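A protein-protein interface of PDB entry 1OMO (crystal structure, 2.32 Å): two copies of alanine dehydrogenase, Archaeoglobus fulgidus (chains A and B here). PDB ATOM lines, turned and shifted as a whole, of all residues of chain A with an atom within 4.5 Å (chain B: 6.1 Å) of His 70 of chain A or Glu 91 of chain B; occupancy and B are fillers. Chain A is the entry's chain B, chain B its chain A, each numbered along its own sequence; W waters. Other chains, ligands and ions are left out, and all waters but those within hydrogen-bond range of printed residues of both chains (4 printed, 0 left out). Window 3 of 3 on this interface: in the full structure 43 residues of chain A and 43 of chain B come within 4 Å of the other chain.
The side-chain amide nitrogen of Asn 73 of chain A lies within hydrogen-bond range of the backbone carbonyl oxygen of Thr 92 of chain B. O of Glu 91 of chain B lies within hydrogen-bond range of ND1 of His 70 of chain A. O of Thr 92 of chain B lies within hydrogen-bond range of ND2 of Asn 68 of chain A (3.2 Å).
Hydrophobic or aromatic side chains of chain B that line the printed part of chain A: Pro 90. Hydrophobic or aromatic side chains of chain A within 4 Å of the printed part of chain B: Phe 46 and His 70. Among the printed residues, no Asp or Glu carboxylate lies within 4 Å of a Lys or Arg side-chain nitrogen of the other chain.
O of Asp 50 of chain A sits at hydrogen-bond distance from NE2 of His 70 of chain A, at 3.4 Å. The backbone NH (N) of His 70 of chain A lies within hydrogen-bond range of the backbone carbonyl oxygen (O) of Thr 80 of chain A. ND1 of His 70 of chain A lies within hydrogen-bond range of O of Lys 48 of chain A (3.2 Å). OG of Ser 89 of chain B is in hydrogen-bond range of OG1 of Thr 92 of chain B (3.2 Å). The side-chain hydroxyl (OG) of Ser 89 of chain B sits close to the backbone NH (N) of Glu 91 of chain B, 3.2 Å away. The backbone NH (N) of Phe 94 of chain B sits close to the side-chain hydroxyl (OG1) of Thr 92 of chain B (3.3 Å).
Among the printed residues, pairs that only touch across the chains: His 70 of chain A with Pro 90 of chain B (2.9 Å), His 70 of chain A with Thr 92 of chain B (3.7 Å), Phe 46 of chain A with Pro 90 of chain B (3.7 Å), Asn 68 of chain A with Gly 93 of chain B (3.7 Å) and His 70 of chain A with Gly 93 of chain B (3.7 Å).
Printed residues of chain B within 4 Å of Phe 46 of chain A: Pro 90 (3.7 Å). Pro 71 of chain A touches none of the printed residues of chain B. Glu 91 of chain B touches just one residue of chain A: His 70. Printed residues of chain A within 4 Å of Gly 93 of chain B: Asn 68 and His 70. Phe 94 of chain B touches none of the printed residues of chain A. The nearest residue of chain B that does not touch His 70 of chain A is Ser 89 of chain B (4.6 Å).
No position is printed for both chains. Of the 8 pairs that touch across the chains among the printed residues, none has its exchanged pair printed and touching as well.
Water W4 bridges the backbone NH of Lys 48 of chain A and the backbone carbonyl oxygen of Pro 90 of chain B. Water W3 bridges OD1 of Asn 73 of chain A (2.6 Å) and O of Glu 91 of chain B (2.6 Å). Water W1 bridges the backbone carbonyl oxygen of Gly 93 of chain B (2.6 Å) and the side-chain amide oxygen of Asn 68 of chain A (2.9 Å). Water W2 bridges the side-chain carboxylate of Glu 91 of chain B (2.9 Å) and the side-chain amino group of Lys 48 of chain A (3.1 Å).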
ATOM      1  N   PHE A  46       9.356  10.978  33.516  1.00  0.00           N
ATOM      2  CA  PHE A  46       9.762   9.764  32.857  1.00  0.00           C
ATOM      3  C   PHE A  46      11.164   9.945  32.353  1.00  0.00           C
ATOM      4  O   PHE A  46      11.703  11.055  32.325  1.00  0.00           O
ATOM      5  CB  PHE A  46       8.869   9.470  31.687  1.00  0.00           C
ATOM      6  CG  PHE A  46       7.435   9.567  32.008  1.00  0.00           C
ATOM      7  CD1 PHE A  46       6.685  10.621  31.519  1.00  0.00           C
ATOM      8  CD2 PHE A  46       6.820   8.590  32.778  1.00  0.00           C
ATOM      9  CE1 PHE A  46       5.328  10.703  31.787  1.00  0.00           C
ATOM     10  CE2 PHE A  46       5.470   8.655  33.056  1.00  0.00           C
ATOM     11  CZ  PHE A  46       4.711   9.718  32.558  1.00  0.00           C
ATOM     12  N   LYS A  48      12.297   9.766  29.289  1.00  0.00           N
ATOM     13  CA  LYS A  48      12.278  10.692  28.156  1.00  0.00           C
ATOM     14  C   LYS A  48      11.231  11.823  28.101  1.00  0.00           C
ATOM     15  O   LYS A  48      10.850  12.239  27.008  1.00  0.00           O
ATOM     16  CB  LYS A  48      12.186   9.879  26.872  1.00  0.00           C
ATOM     17  CG  LYS A  48      13.230   8.789  26.785  1.00  0.00           C
ATOM     18  CD  LYS A  48      12.915   7.831  25.662  1.00  0.00           C
ATOM     19  CE  LYS A  48      13.777   6.585  25.748  1.00  0.00           C
ATOM     20  NZ  LYS A  48      13.017   5.416  25.194  1.00  0.00           N
ATOM     21  N   GLY A  49      10.784  12.338  29.243  1.00  0.00           N
ATOM     22  CA  GLY A  49       9.801  13.408  29.226  1.00  0.00           C
ATOM     23  C   GLY A  49       8.930  13.354  30.471  1.00  0.00           C
ATOM     24  O   GLY A  49       9.302  12.708  31.461  1.00  0.00           O
ATOM     25  N   ASP A  50       7.773  14.015  30.453  1.00  0.00           N
ATOM     26  CA  ASP A  50       6.903  13.986  31.632  1.00  0.00           C
ATOM     27  C   ASP A  50       5.433  14.193  31.274  1.00  0.00           C
ATOM     28  O   ASP A  50       5.069  14.255  30.104  1.00  0.00           O
ATOM     29  CB  ASP A  50       7.347  15.050  32.657  1.00  0.00           C
ATOM     30  CG  ASP A  50       6.995  16.478  32.233  1.00  0.00           C
ATOM     31  OD1 ASP A  50       6.398  16.673  31.152  1.00  0.00           O
ATOM     32  OD2 ASP A  50       7.316  17.416  32.997  1.00  0.00           O
ATOM     33  N   ASN A  68       1.765  16.373  28.336  1.00  0.00           N
ATOM     34  CA  ASN A  68       3.124  15.841  28.361  1.00  0.00           C
ATOM     35  C   ASN A  68       4.156  16.714  27.624  1.00  0.00           C
ATOM     36  O   ASN A  68       3.836  17.737  27.000  1.00  0.00           O
ATOM     37  CB  ASN A  68       3.157  14.478  27.671  1.00  0.00           C
ATOM     38  CG  ASN A  68       3.181  14.614  26.152  1.00  0.00           C
ATOM     39  OD1 ASN A  68       2.203  15.067  25.553  1.00  0.00           O
ATOM     40  ND2 ASN A  68       4.304  14.245  25.521  1.00  0.00           N
ATOM     41  N   SER A  69       5.399  16.257  27.678  1.00  0.00           N
ATOM     42  CA  SER A  69       6.513  16.903  26.993  1.00  0.00           C
ATOM     43  C   SER A  69       7.635  15.883  26.803  1.00  0.00           C
ATOM     44  O   SER A  69       8.386  15.609  27.732  1.00  0.00           O
ATOM     45  CB  SER A  69       7.061  18.069  27.789  1.00  0.00           C
ATOM     46  OG  SER A  69       8.100  18.659  27.046  1.00  0.00           O
ATOM     47  N   HIS A  70       7.726  15.306  25.614  1.00  0.00           N
ATOM     48  CA  HIS A  70       8.767  14.323  25.319  1.00  0.00           C
ATOM     49  C   HIS A  70       9.644  14.759  24.142  1.00  0.00           C
ATOM     50  O   HIS A  70       9.456  14.316  23.011  1.00  0.00           O
ATOM     51  CB  HIS A  70       8.125  12.966  25.045  1.00  0.00           C
ATOM     52  CG  HIS A  70       7.519  12.353  26.266  1.00  0.00           C
ATOM     53  ND1 HIS A  70       7.895  11.117  26.743  1.00  0.00           N
ATOM     54  CD2 HIS A  70       6.625  12.847  27.159  1.00  0.00           C
ATOM     55  CE1 HIS A  70       7.263  10.880  27.880  1.00  0.00           C
ATOM     56  NE2 HIS A  70       6.487  11.914  28.152  1.00  0.00           N
ATOM     57  N   PRO A  71      10.639  15.614  24.423  1.00  0.00           N
ATOM     58  CA  PRO A  71      11.604  16.190  23.478  1.00  0.00           C
ATOM     59  C   PRO A  71      12.043  15.323  22.306  1.00  0.00           C
ATOM     60  O   PRO A  71      12.329  15.842  21.232  1.00  0.00           O
ATOM     61  CB  PRO A  71      12.764  16.585  24.378  1.00  0.00           C
ATOM     62  CG  PRO A  71      12.068  16.987  25.653  1.00  0.00           C
ATOM     63  CD  PRO A  71      11.098  15.828  25.810  1.00  0.00           C
ATOM     64  N   GLY A  72      12.100  14.013  22.493  1.00  0.00           N
ATOM     65  CA  GLY A  72      12.507  13.156  21.396  1.00  0.00           C
ATOM     66  C   GLY A  72      11.338  12.650  20.571  1.00  0.00           C
ATOM     67  O   GLY A  72      11.447  11.665  19.830  1.00  0.00           O
ATOM     68  N   ASN A  73      10.210  13.341  20.676  1.00  0.00           N
ATOM     69  CA  ASN A  73       9.006  12.948  19.961  1.00  0.00           C
ATOM     70  C   ASN A  73       8.941  13.311  18.463  1.00  0.00           C
ATOM     71  O   ASN A  73       8.541  12.483  17.642  1.00  0.00           O
ATOM     72  CB  ASN A  73       7.789  13.506  20.711  1.00  0.00           C
ATOM     73  CG  ASN A  73       7.067  12.435  21.549  1.00  0.00           C
ATOM     74  OD1 ASN A  73       7.606  11.355  21.817  1.00  0.00           O
ATOM     75  ND2 ASN A  73       5.843  12.747  21.967  1.00  0.00           N
ATOM     76  N   PRO A  74       9.337  14.544  18.091  1.00  0.00           N
ATOM     77  CA  PRO A  74       9.290  14.940  16.676  1.00  0.00           C
ATOM     78  C   PRO A  74      10.110  14.005  15.812  1.00  0.00           C
ATOM     79  O   PRO A  74       9.627  13.480  14.804  1.00  0.00           O
ATOM     80  CB  PRO A  74       9.855  16.356  16.693  1.00  0.00           C
ATOM     81  CG  PRO A  74      10.837  16.297  17.798  1.00  0.00           C
ATOM     82  CD  PRO A  74      10.063  15.551  18.880  1.00  0.00           C
ATOM     83  N   THR A  80       6.111  17.147  20.257  1.00  0.00           N
ATOM     84  CA  THR A  80       6.672  17.007  21.599  1.00  0.00           C
ATOM     85  C   THR A  80       5.600  17.185  22.665  1.00  0.00           C
ATOM     86  O   THR A  80       5.655  16.565  23.735  1.00  0.00           O
ATOM     87  CB  THR A  80       7.756  18.062  21.868  1.00  0.00           C
ATOM     88  OG1 THR A  80       8.827  17.871  20.940  1.00  0.00           O
ATOM     89  CG2 THR A  80       8.294  17.938  23.292  1.00  0.00           C
ATOM     90  N   GLY B  60       4.593  -0.113  33.161  1.00  0.00           N
ATOM     91  CA  GLY B  60       4.773   0.334  31.803  1.00  0.00           C
ATOM     92  C   GLY B  60       3.811   1.361  31.258  1.00  0.00           C
ATOM     93  O   GLY B  60       3.902   1.724  30.081  1.00  0.00           O
ATOM     94  N   SER B  89       1.293   6.727  27.186  1.00  0.00           N
ATOM     95  CA  SER B  89       2.527   5.970  26.976  1.00  0.00           C
ATOM     96  C   SER B  89       3.643   6.731  27.684  1.00  0.00           C
ATOM     97  O   SER B  89       3.810   7.920  27.469  1.00  0.00           O
ATOM     98  CB  SER B  89       2.854   5.877  25.485  1.00  0.00           C
ATOM     99  OG  SER B  89       4.239   5.640  25.281  1.00  0.00           O
ATOM    100  N   PRO B  90       4.415   6.063  28.544  1.00  0.00           N
ATOM    101  CA  PRO B  90       5.486   6.806  29.206  1.00  0.00           C
ATOM    102  C   PRO B  90       6.643   7.199  28.250  1.00  0.00           C
ATOM    103  O   PRO B  90       7.430   8.099  28.560  1.00  0.00           O
ATOM    104  CB  PRO B  90       5.949   5.847  30.306  1.00  0.00           C
ATOM    105  CG  PRO B  90       4.747   4.976  30.566  1.00  0.00           C
ATOM    106  CD  PRO B  90       4.256   4.729  29.145  1.00  0.00           C
ATOM    107  N   GLU B  91       6.761   6.544  27.101  1.00  0.00           N
ATOM    108  CA  GLU B  91       7.853   6.877  26.184  1.00  0.00           C
ATOM    109  C   GLU B  91       7.545   8.052  25.271  1.00  0.00           C
ATOM    110  O   GLU B  91       8.465   8.773  24.863  1.00  0.00           O
ATOM    111  CB  GLU B  91       8.234   5.675  25.315  1.00  0.00           C
ATOM    112  CG  GLU B  91       9.133   4.650  26.007  1.00  0.00           C
ATOM    113  CD  GLU B  91       8.427   3.917  27.140  1.00  0.00           C
ATOM    114  OE1 GLU B  91       7.379   3.269  26.884  1.00  0.00           O
ATOM    115  OE2 GLU B  91       8.921   3.988  28.293  1.00  0.00           O
ATOM    116  N   THR B  92       6.265   8.263  24.963  1.00  0.00           N
ATOM    117  CA  THR B  92       5.857   9.351  24.069  1.00  0.00           C
ATOM    118  C   THR B  92       4.848  10.336  24.681  1.00  0.00           C
ATOM    119  O   THR B  92       4.581  11.390  24.103  1.00  0.00           O
ATOM    120  CB  THR B  92       5.210   8.779  22.820  1.00  0.00           C
ATOM    121  OG1 THR B  92       4.025   8.063  23.199  1.00  0.00           O
ATOM    122  CG2 THR B  92       6.163   7.820  22.112  1.00  0.00           C
ATOM    123  N   GLY B  93       4.274   9.968  25.834  1.00  0.00           N
ATOM    124  CA  GLY B  93       3.285  10.801  26.507  1.00  0.00           C
ATOM    125  C   GLY B  93       1.936  10.739  25.811  1.00  0.00           C
ATOM    126  O   GLY B  93       0.956  11.328  26.254  1.00  0.00           O
ATOM    127  N   PHE B  94       1.878  10.008  24.711  1.00  0.00           N
ATOM    128  CA  PHE B  94       0.659   9.909  23.941  1.00  0.00           C
ATOM    129  C   PHE B  94      -0.519   9.311  24.714  1.00  0.00           C
ATOM    130  O   PHE B  94      -0.373   8.310  25.443  1.00  0.00           O
ATOM    131  CB  PHE B  94       0.900   9.078  22.690  1.00  0.00           C
ATOM    132  CG  PHE B  94      -0.286   9.032  21.757  1.00  0.00           C
ATOM    133  CD1 PHE B  94      -0.536  10.078  20.883  1.00  0.00           C
ATOM    134  CD2 PHE B  94      -1.169   7.966  21.780  1.00  0.00           C
ATOM    135  CE1 PHE B  94      -1.646  10.071  20.047  1.00  0.00           C
ATOM    136  CE2 PHE B  94      -2.292   7.938  20.944  1.00  0.00           C
ATOM    137  CZ  PHE B  94      -2.531   8.995  20.078  1.00  0.00           C
HETATM  138  O   HOH W   1      -0.208  13.675  26.432  1.00  0.00           O
HETATM  139  O   HOH W   2      11.658   4.945  27.986  1.00  0.00           O
HETATM  140  O   HOH W   3       9.603  10.370  23.145  1.00  0.00           O
HETATM  141  O   HOH W   4      10.468   8.252  28.396  1.00  0.00           O
